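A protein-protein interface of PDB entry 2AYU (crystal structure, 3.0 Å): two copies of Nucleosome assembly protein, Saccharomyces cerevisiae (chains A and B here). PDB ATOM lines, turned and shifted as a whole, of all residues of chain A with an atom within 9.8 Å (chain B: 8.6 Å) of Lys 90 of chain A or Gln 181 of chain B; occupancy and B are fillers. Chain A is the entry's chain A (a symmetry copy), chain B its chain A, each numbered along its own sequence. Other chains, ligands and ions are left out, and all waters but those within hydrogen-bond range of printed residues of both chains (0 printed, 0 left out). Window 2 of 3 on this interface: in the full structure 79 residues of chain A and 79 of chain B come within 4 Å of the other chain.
Among the printed residues, merely in contact across the chains: Val 85 of chain A with Leu 165 of chain B (3.2 Å), Pro 89 of chain A with Gln 181 of chain B (3.3 Å), Lys 90 of chain A with Gln 181 of chain B (3.7 Å), Asn 91 of chain A with Gln 181 of chain B (3.0 Å), Val 92 of chain A with Val 182 of chain B (3.5 Å), Val 92 of chain A with Gly 184 of chain B (3.8 Å), Lys 93 of chain A with Leu 165 of chain B (3.9 Å), Lys 93 of chain A with Leu 166 of chain B (3.6 Å), Lys 93 of chain A with Val 167 of chain B (3.5 Å), Glu 94 of chain A with Ile 150 of chain B (3.0 Å), Lys 95 of chain A with Pro 145 of chain B (3.8 Å), Lys 95 of chain A with Gly 184 of chain B (3.4 Å), Leu 96 of chain A with Leu 165 of chain B (3.7 Å), Leu 97 of chain A with Ile 150 of chain B (3.7 Å), Leu 97 of chain A with Leu 165 of chain B (2.9 Å), Leu 97 of chain A with Val 167 of chain B (3.4 Å) and Ser 98 of chain A with Pro 145 of chain B (3.6 Å).
Of the 14 printed residues of chain B, 9 touch a printed residue of chain A. Printed residues of chain B that touch a printed residue of chain A: Pro 145, Ile 150, Leu 165, Leu 166, Val 167, Glu 171, Gln 181, Val 182 and Gly 184. Of the 14 printed residues of chain A, 11 touch a printed residue of chain B. Printed residues of chain A that touch a printed residue of chain B: Val 85, Pro 89, Lys 90, Asn 91, Val 92, Lys 93, Glu 94, Lys 95, Leu 96, Leu 97 and Ser 98.
No position is printed for both chains. Of the 19 pairs that touch across the chains among the printed residues, none has its exchanged pair printed and touching as well.
O of Lys 95 of chain A lies within hydrogen-bond range of OG of Ser 98 of chain A (2.4 Å). NZ of Lys 95 of chain A lies close to ND2 of Asn 91 of chain A, 3.2 Å away. O of Leu 88 of chain A sits at hydrogen-bond distance from NZ of Lys 93 of chain A, at 2.7 Å. The backbone carbonyl oxygen of Gly 86 of chain A lies within hydrogen-bond range of the side-chain amino group of Lys 93 of chain A.
The side-chain carboxylate (OE2) of Glu 171 of chain B sits close to the side-chain carboxylate (OE2) of Glu 94 of chain A, 2.7 Å away. OD1 of Asn 91 of chain A sits close to O of Val 182 of chain B, 2.8 Å away.
Lys 90 of chain A touches one residue of chain B. Val 182 of chain B touches just these residues of chain A: Asn 91 and Val 92. Of the printed residues of chain B, Leu 96 of chain A touches Leu 165. Printed residues of chain B within 4 Å of Val 92 of chain A: Val 182 and Gly 184. Of the printed residues of chain A, Leu 166 of chain B touches Lys 93. Of the printed residues of chain A, Ile 150 of chain B touches Glu 94 and Leu 97. Of the printed residues of chain B, Val 85 of chain A touches Leu 165 (3.2 Å). The nearest residue of chain B that does not touch Lys 90 of chain A is Val 167 of chain B (4.2 Å). The nearest printed residue of chain A that does not touch Ile 150 of chain B is Lys 95 of chain A (4.3 Å).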
ATOM      1  N   VAL A  85      -6.792  -0.020  -7.665  1.00  0.00           N
ATOM      2  CA  VAL A  85      -6.751   0.889  -6.524  1.00  0.00           C
ATOM      3  C   VAL A  85      -5.395   1.548  -6.420  1.00  0.00           C
ATOM      4  O   VAL A  85      -5.298   2.738  -6.112  1.00  0.00           O
ATOM      5  CB  VAL A  85      -7.060   0.153  -5.194  1.00  0.00           C
ATOM      6  CG1 VAL A  85      -6.342  -1.164  -5.159  1.00  0.00           C
ATOM      7  CG2 VAL A  85      -6.621   1.004  -4.001  1.00  0.00           C
ATOM      8  N   GLY A  86      -4.348   0.771  -6.677  1.00  0.00           N
ATOM      9  CA  GLY A  86      -3.009   1.319  -6.617  1.00  0.00           C
ATOM     10  C   GLY A  86      -2.836   2.489  -7.577  1.00  0.00           C
ATOM     11  O   GLY A  86      -2.111   3.444  -7.280  1.00  0.00           O
ATOM     12  N   GLY A  87      -3.513   2.423  -8.725  1.00  0.00           N
ATOM     13  CA  GLY A  87      -3.404   3.480  -9.718  1.00  0.00           C
ATOM     14  C   GLY A  87      -4.297   4.700  -9.554  1.00  0.00           C
ATOM     15  O   GLY A  87      -4.106   5.699 -10.243  1.00  0.00           O
ATOM     16  N   LEU A  88      -5.272   4.639  -8.656  1.00  0.00           N
ATOM     17  CA  LEU A  88      -6.169   5.771  -8.454  1.00  0.00           C
ATOM     18  C   LEU A  88      -5.411   7.057  -8.068  1.00  0.00           C
ATOM     19  O   LEU A  88      -4.283   7.004  -7.561  1.00  0.00           O
ATOM     20  CB  LEU A  88      -7.209   5.421  -7.382  1.00  0.00           C
ATOM     21  CG  LEU A  88      -8.045   4.151  -7.586  1.00  0.00           C
ATOM     22  CD1 LEU A  88      -9.027   4.005  -6.432  1.00  0.00           C
ATOM     23  CD2 LEU A  88      -8.797   4.213  -8.906  1.00  0.00           C
ATOM     24  N   PRO A  89      -6.024   8.232  -8.323  1.00  0.00           N
ATOM     25  CA  PRO A  89      -5.470   9.562  -8.031  1.00  0.00           C
ATOM     26  C   PRO A  89      -5.181   9.774  -6.552  1.00  0.00           C
ATOM     27  O   PRO A  89      -5.766   9.098  -5.706  1.00  0.00           O
ATOM     28  CB  PRO A  89      -6.565  10.506  -8.518  1.00  0.00           C
ATOM     29  CG  PRO A  89      -7.192   9.746  -9.629  1.00  0.00           C
ATOM     30  CD  PRO A  89      -7.293   8.355  -9.060  1.00  0.00           C
ATOM     31  N   LYS A  90      -4.275  10.708  -6.249  1.00  0.00           N
ATOM     32  CA  LYS A  90      -3.923  11.056  -4.862  1.00  0.00           C
ATOM     33  C   LYS A  90      -5.271  11.368  -4.209  1.00  0.00           C
ATOM     34  O   LYS A  90      -5.667  10.798  -3.178  1.00  0.00           O
ATOM     35  CB  LYS A  90      -3.055  12.325  -4.847  1.00  0.00           C
ATOM     36  CG  LYS A  90      -3.663  13.477  -5.678  1.00  0.00           C
ATOM     37  CD  LYS A  90      -3.010  14.844  -5.451  1.00  0.00           C
ATOM     38  CE  LYS A  90      -3.697  15.915  -6.313  1.00  0.00           C
ATOM     39  NZ  LYS A  90      -3.079  17.270  -6.199  1.00  0.00           N
ATOM     40  N   ASN A  91      -5.946  12.301  -4.871  1.00  0.00           N
ATOM     41  CA  ASN A  91      -7.261  12.806  -4.539  1.00  0.00           C
ATOM     42  C   ASN A  91      -8.137  11.658  -4.055  1.00  0.00           C
ATOM     43  O   ASN A  91      -8.431  11.548  -2.866  1.00  0.00           O
ATOM     44  CB  ASN A  91      -7.829  13.443  -5.809  1.00  0.00           C
ATOM     45  CG  ASN A  91      -9.247  13.882  -5.658  1.00  0.00           C
ATOM     46  OD1 ASN A  91     -10.074  13.592  -6.518  1.00  0.00           O
ATOM     47  ND2 ASN A  91      -9.547  14.599  -4.576  1.00  0.00           N
ATOM     48  N   VAL A  92      -8.529  10.794  -4.988  1.00  0.00           N
ATOM     49  CA  VAL A  92      -9.381   9.642  -4.690  1.00  0.00           C
ATOM     50  C   VAL A  92      -8.813   8.710  -3.624  1.00  0.00           C
ATOM     51  O   VAL A  92      -9.531   8.297  -2.708  1.00  0.00           O
ATOM     52  CB  VAL A  92      -9.637   8.807  -5.952  1.00  0.00           C
ATOM     53  CG1 VAL A  92     -10.388   7.547  -5.583  1.00  0.00           C
ATOM     54  CG2 VAL A  92     -10.420   9.630  -6.969  1.00  0.00           C
ATOM     55  N   LYS A  93      -7.534   8.366  -3.774  1.00  0.00           N
ATOM     56  CA  LYS A  93      -6.837   7.490  -2.837  1.00  0.00           C
ATOM     57  C   LYS A  93      -7.125   7.930  -1.414  1.00  0.00           C
ATOM     58  O   LYS A  93      -7.491   7.121  -0.555  1.00  0.00           O
ATOM     59  CB  LYS A  93      -5.325   7.552  -3.064  1.00  0.00           C
ATOM     60  CG  LYS A  93      -4.750   6.422  -3.884  1.00  0.00           C
ATOM     61  CD  LYS A  93      -3.248   6.344  -3.664  1.00  0.00           C
ATOM     62  CE  LYS A  93      -2.630   5.213  -4.458  1.00  0.00           C
ATOM     63  NZ  LYS A  93      -2.882   5.412  -5.911  1.00  0.00           N
ATOM     64  N   GLU A  94      -6.945   9.223  -1.174  1.00  0.00           N
ATOM     65  CA  GLU A  94      -7.174   9.809   0.139  1.00  0.00           C
ATOM     66  C   GLU A  94      -8.548   9.464   0.716  1.00  0.00           C
ATOM     67  O   GLU A  94      -8.646   8.955   1.840  1.00  0.00           O
ATOM     68  CB  GLU A  94      -7.010  11.324   0.054  1.00  0.00           C
ATOM     69  CG  GLU A  94      -5.645  11.758  -0.428  1.00  0.00           C
ATOM     70  CD  GLU A  94      -5.292  13.139   0.057  1.00  0.00           C
ATOM     71  OE1 GLU A  94      -5.323  13.352   1.289  1.00  0.00           O
ATOM     72  OE2 GLU A  94      -4.983  14.006  -0.790  1.00  0.00           O
ATOM     73  N   LYS A  95      -9.593   9.758  -0.059  1.00  0.00           N
ATOM     74  CA  LYS A  95     -10.978   9.479   0.321  1.00  0.00           C
ATOM     75  C   LYS A  95     -11.085   8.068   0.936  1.00  0.00           C
ATOM     76  O   LYS A  95     -11.653   7.877   2.021  1.00  0.00           O
ATOM     77  CB  LYS A  95     -11.863   9.552  -0.923  1.00  0.00           C
ATOM     78  CG  LYS A  95     -11.779  10.838  -1.708  1.00  0.00           C
ATOM     79  CD  LYS A  95     -12.834  11.839  -1.253  1.00  0.00           C
ATOM     80  CE  LYS A  95     -13.002  13.000  -2.257  1.00  0.00           C
ATOM     81  NZ  LYS A  95     -11.760  13.820  -2.469  1.00  0.00           N
ATOM     82  N   LEU A  96     -10.543   7.083   0.221  1.00  0.00           N
ATOM     83  CA  LEU A  96     -10.551   5.694   0.668  1.00  0.00           C
ATOM     84  C   LEU A  96      -9.788   5.555   1.980  1.00  0.00           C
ATOM     85  O   LEU A  96     -10.192   4.795   2.857  1.00  0.00           O
ATOM     86  CB  LEU A  96      -9.933   4.786  -0.406  1.00  0.00           C
ATOM     87  CG  LEU A  96     -10.755   4.431  -1.653  1.00  0.00           C
ATOM     88  CD1 LEU A  96     -11.171   5.686  -2.388  1.00  0.00           C
ATOM     89  CD2 LEU A  96      -9.921   3.550  -2.558  1.00  0.00           C
ATOM     90  N   LEU A  97      -8.681   6.279   2.109  1.00  0.00           N
ATOM     91  CA  LEU A  97      -7.915   6.228   3.343  1.00  0.00           C
ATOM     92  C   LEU A  97      -8.843   6.543   4.518  1.00  0.00           C
ATOM     93  O   LEU A  97      -8.769   5.900   5.569  1.00  0.00           O
ATOM     94  CB  LEU A  97      -6.766   7.244   3.331  1.00  0.00           C
ATOM     95  CG  LEU A  97      -5.366   6.819   2.863  1.00  0.00           C
ATOM     96  CD1 LEU A  97      -5.129   5.342   3.175  1.00  0.00           C
ATOM     97  CD2 LEU A  97      -5.227   7.081   1.382  1.00  0.00           C
ATOM     98  N   SER A  98      -9.718   7.533   4.333  1.00  0.00           N
ATOM     99  CA  SER A  98     -10.658   7.939   5.386  1.00  0.00           C
ATOM    100  C   SER A  98     -11.798   6.937   5.506  1.00  0.00           C
ATOM    101  O   SER A  98     -12.335   6.702   6.592  1.00  0.00           O
ATOM    102  CB  SER A  98     -11.206   9.347   5.102  1.00  0.00           C
ATOM    103  OG  SER A  98     -11.895   9.396   3.866  1.00  0.00           O
ATOM    104  N   PRO B 145     -12.627  14.550   3.256  1.00  0.00           N
ATOM    105  CA  PRO B 145     -11.942  13.855   4.348  1.00  0.00           C
ATOM    106  C   PRO B 145     -11.136  14.796   5.234  1.00  0.00           C
ATOM    107  O   PRO B 145     -10.311  15.567   4.743  1.00  0.00           O
ATOM    108  CB  PRO B 145     -11.043  12.856   3.617  1.00  0.00           C
ATOM    109  CG  PRO B 145     -11.675  12.734   2.227  1.00  0.00           C
ATOM    110  CD  PRO B 145     -12.078  14.146   1.951  1.00  0.00           C
ATOM    111  N   ILE B 150      -7.738  11.120   7.201  1.00  0.00           N
ATOM    112  CA  ILE B 150      -6.779  10.819   6.155  1.00  0.00           C
ATOM    113  C   ILE B 150      -5.510  10.122   6.663  1.00  0.00           C
ATOM    114  O   ILE B 150      -5.034   9.168   6.039  1.00  0.00           O
ATOM    115  CB  ILE B 150      -6.407  12.113   5.400  1.00  0.00           C
ATOM    116  CG1 ILE B 150      -7.310  12.263   4.185  1.00  0.00           C
ATOM    117  CG2 ILE B 150      -4.941  12.099   4.985  1.00  0.00           C
ATOM    118  CD1 ILE B 150      -7.176  11.114   3.234  1.00  0.00           C
ATOM    119  N   LEU B 165      -2.920   1.799  -1.143  1.00  0.00           N
ATOM    120  CA  LEU B 165      -3.744   2.908  -0.652  1.00  0.00           C
ATOM    121  C   LEU B 165      -2.934   4.046  -0.066  1.00  0.00           C
ATOM    122  O   LEU B 165      -3.425   5.161   0.053  1.00  0.00           O
ATOM    123  CB  LEU B 165      -4.727   2.403   0.411  1.00  0.00           C
ATOM    124  CG  LEU B 165      -6.242   2.396   0.149  1.00  0.00           C
ATOM    125  CD1 LEU B 165      -6.552   2.732  -1.319  1.00  0.00           C
ATOM    126  CD2 LEU B 165      -6.803   1.023   0.553  1.00  0.00           C
ATOM    127  N   LEU B 166      -1.697   3.762   0.316  1.00  0.00           N
ATOM    128  CA  LEU B 166      -0.841   4.791   0.884  1.00  0.00           C
ATOM    129  C   LEU B 166      -0.648   5.937  -0.110  1.00  0.00           C
ATOM    130  O   LEU B 166      -0.601   5.718  -1.329  1.00  0.00           O
ATOM    131  CB  LEU B 166       0.519   4.198   1.264  1.00  0.00           C
ATOM    132  CG  LEU B 166       0.500   3.099   2.334  1.00  0.00           C
ATOM    133  CD1 LEU B 166       1.864   2.435   2.441  1.00  0.00           C
ATOM    134  CD2 LEU B 166       0.077   3.701   3.666  1.00  0.00           C
ATOM    135  N   VAL B 167      -0.558   7.156   0.421  1.00  0.00           N
ATOM    136  CA  VAL B 167      -0.357   8.361  -0.379  1.00  0.00           C
ATOM    137  C   VAL B 167       0.706   9.172   0.360  1.00  0.00           C
ATOM    138  O   VAL B 167       0.725   9.166   1.589  1.00  0.00           O
ATOM    139  CB  VAL B 167      -1.654   9.190  -0.477  1.00  0.00           C
ATOM    140  CG1 VAL B 167      -1.518  10.236  -1.576  1.00  0.00           C
ATOM    141  CG2 VAL B 167      -2.844   8.278  -0.753  1.00  0.00           C
ATOM    142  N   ASP B 168       1.584   9.867  -0.362  1.00  0.00           N
ATOM    143  CA  ASP B 168       2.646  10.635   0.292  1.00  0.00           C
ATOM    144  C   ASP B 168       2.203  11.840   1.104  1.00  0.00           C
ATOM    145  O   ASP B 168       1.061  11.894   1.540  1.00  0.00           O
ATOM    146  CB  ASP B 168       3.705  11.031  -0.726  1.00  0.00           C
ATOM    147  CG  ASP B 168       4.755   9.958  -0.880  1.00  0.00           C
ATOM    148  OD1 ASP B 168       5.560   9.798   0.058  1.00  0.00           O
ATOM    149  OD2 ASP B 168       4.762   9.251  -1.910  1.00  0.00           O
ATOM    150  N   GLU B 169       3.108  12.789   1.336  1.00  0.00           N
ATOM    151  CA  GLU B 169       2.785  13.980   2.128  1.00  0.00           C
ATOM    152  C   GLU B 169       1.300  14.309   2.098  1.00  0.00           C
ATOM    153  O   GLU B 169       0.834  14.937   1.150  1.00  0.00           O
ATOM    154  CB  GLU B 169       3.530  15.198   1.603  1.00  0.00           C
ATOM    155  CG  GLU B 169       5.016  15.070   1.552  1.00  0.00           C
ATOM    156  CD  GLU B 169       5.625  16.270   0.879  1.00  0.00           C
ATOM    157  OE1 GLU B 169       5.205  16.563  -0.258  1.00  0.00           O
ATOM    158  OE2 GLU B 169       6.510  16.922   1.473  1.00  0.00           O
ATOM    159  N   GLU B 170       0.556  13.888   3.120  1.00  0.00           N
ATOM    160  CA  GLU B 170      -0.878  14.172   3.159  1.00  0.00           C
ATOM    161  C   GLU B 170      -1.063  15.681   3.103  1.00  0.00           C
ATOM    162  O   GLU B 170      -0.235  16.439   3.628  1.00  0.00           O
ATOM    163  CB  GLU B 170      -1.512  13.640   4.443  1.00  0.00           C
ATOM    164  CG  GLU B 170      -1.480  12.132   4.613  1.00  0.00           C
ATOM    165  CD  GLU B 170      -1.606  11.719   6.076  1.00  0.00           C
ATOM    166  OE1 GLU B 170      -2.434  12.322   6.793  1.00  0.00           O
ATOM    167  OE2 GLU B 170      -0.878  10.794   6.506  1.00  0.00           O
ATOM    168  N   GLU B 171      -2.153  16.101   2.465  1.00  0.00           N
ATOM    169  CA  GLU B 171      -2.496  17.514   2.297  1.00  0.00           C
ATOM    170  C   GLU B 171      -2.087  18.368   3.499  1.00  0.00           C
ATOM    171  O   GLU B 171      -0.938  18.796   3.615  1.00  0.00           O
ATOM    172  CB  GLU B 171      -4.007  17.649   2.064  1.00  0.00           C
ATOM    173  CG  GLU B 171      -4.579  16.715   0.993  1.00  0.00           C
ATOM    174  CD  GLU B 171      -4.183  17.106  -0.417  1.00  0.00           C
ATOM    175  OE1 GLU B 171      -4.538  18.224  -0.839  1.00  0.00           O
ATOM    176  OE2 GLU B 171      -3.522  16.296  -1.101  1.00  0.00           O
ATOM    177  N   GLN B 181      -8.851  17.640  -9.629  1.00  0.00           N
ATOM    178  CA  GLN B 181      -9.242  16.409 -10.307  1.00  0.00           C
ATOM    179  C   GLN B 181     -10.729  16.075 -10.090  1.00  0.00           C
ATOM    180  O   GLN B 181     -11.581  16.969 -10.070  1.00  0.00           O
ATOM    181  CB  GLN B 181      -8.367  15.251  -9.818  1.00  0.00           C
ATOM    182  CG  GLN B 181      -6.880  15.563  -9.837  1.00  0.00           C
ATOM    183  CD  GLN B 181      -6.038  14.400  -9.368  1.00  0.00           C
ATOM    184  OE1 GLN B 181      -6.283  13.831  -8.302  1.00  0.00           O
ATOM    185  NE2 GLN B 181      -5.036  14.040 -10.161  1.00  0.00           N
ATOM    186  N   VAL B 182     -11.029  14.788  -9.921  1.00  0.00           N
ATOM    187  CA  VAL B 182     -12.403  14.320  -9.718  1.00  0.00           C
ATOM    188  C   VAL B 182     -13.010  14.635  -8.345  1.00  0.00           C
ATOM    189  O   VAL B 182     -12.302  14.979  -7.398  1.00  0.00           O
ATOM    190  CB  VAL B 182     -12.498  12.793  -9.951  1.00  0.00           C
ATOM    191  CG1 VAL B 182     -12.514  12.499 -11.448  1.00  0.00           C
ATOM    192  CG2 VAL B 182     -11.308  12.082  -9.279  1.00  0.00           C
ATOM    193  N   LYS B 183     -14.333  14.524  -8.247  1.00  0.00           N
ATOM    194  CA  LYS B 183     -15.020  14.781  -6.984  1.00  0.00           C
ATOM    195  C   LYS B 183     -15.449  13.470  -6.338  1.00  0.00           C
ATOM    196  O   LYS B 183     -16.061  12.616  -6.982  1.00  0.00           O
ATOM    197  CB  LYS B 183     -16.242  15.682  -7.193  1.00  0.00           C
ATOM    198  CG  LYS B 183     -16.089  17.073  -6.567  1.00  0.00           C
ATOM    199  CD  LYS B 183     -15.860  17.009  -5.047  1.00  0.00           C
ATOM    200  CE  LYS B 183     -15.550  18.387  -4.467  1.00  0.00           C
ATOM    201  NZ  LYS B 183     -16.619  19.377  -4.769  1.00  0.00           N
ATOM    202  N   GLY B 184     -15.126  13.318  -5.059  1.00  0.00           N
ATOM    203  CA  GLY B 184     -15.474  12.096  -4.364  1.00  0.00           C
ATOM    204  C   GLY B 184     -14.716  10.928  -4.968  1.00  0.00           C
ATOM    205  O   GLY B 184     -13.573  11.084  -5.408  1.00  0.00           O
ATOM    206  N   PRO B 186     -15.540   8.065  -7.787  1.00  0.00           N
ATOM    207  CA  PRO B 186     -16.324   7.538  -8.907  1.00  0.00           C
ATOM    208  C   PRO B 186     -16.571   6.050  -8.873  1.00  0.00           C
ATOM    209  O   PRO B 186     -15.764   5.309  -8.337  1.00  0.00           O
ATOM    210  CB  PRO B 186     -15.490   7.918 -10.114  1.00  0.00           C
ATOM    211  CG  PRO B 186     -14.825   9.159  -9.674  1.00  0.00           C
ATOM    212  CD  PRO B 186     -14.392   8.838  -8.287  1.00  0.00           C
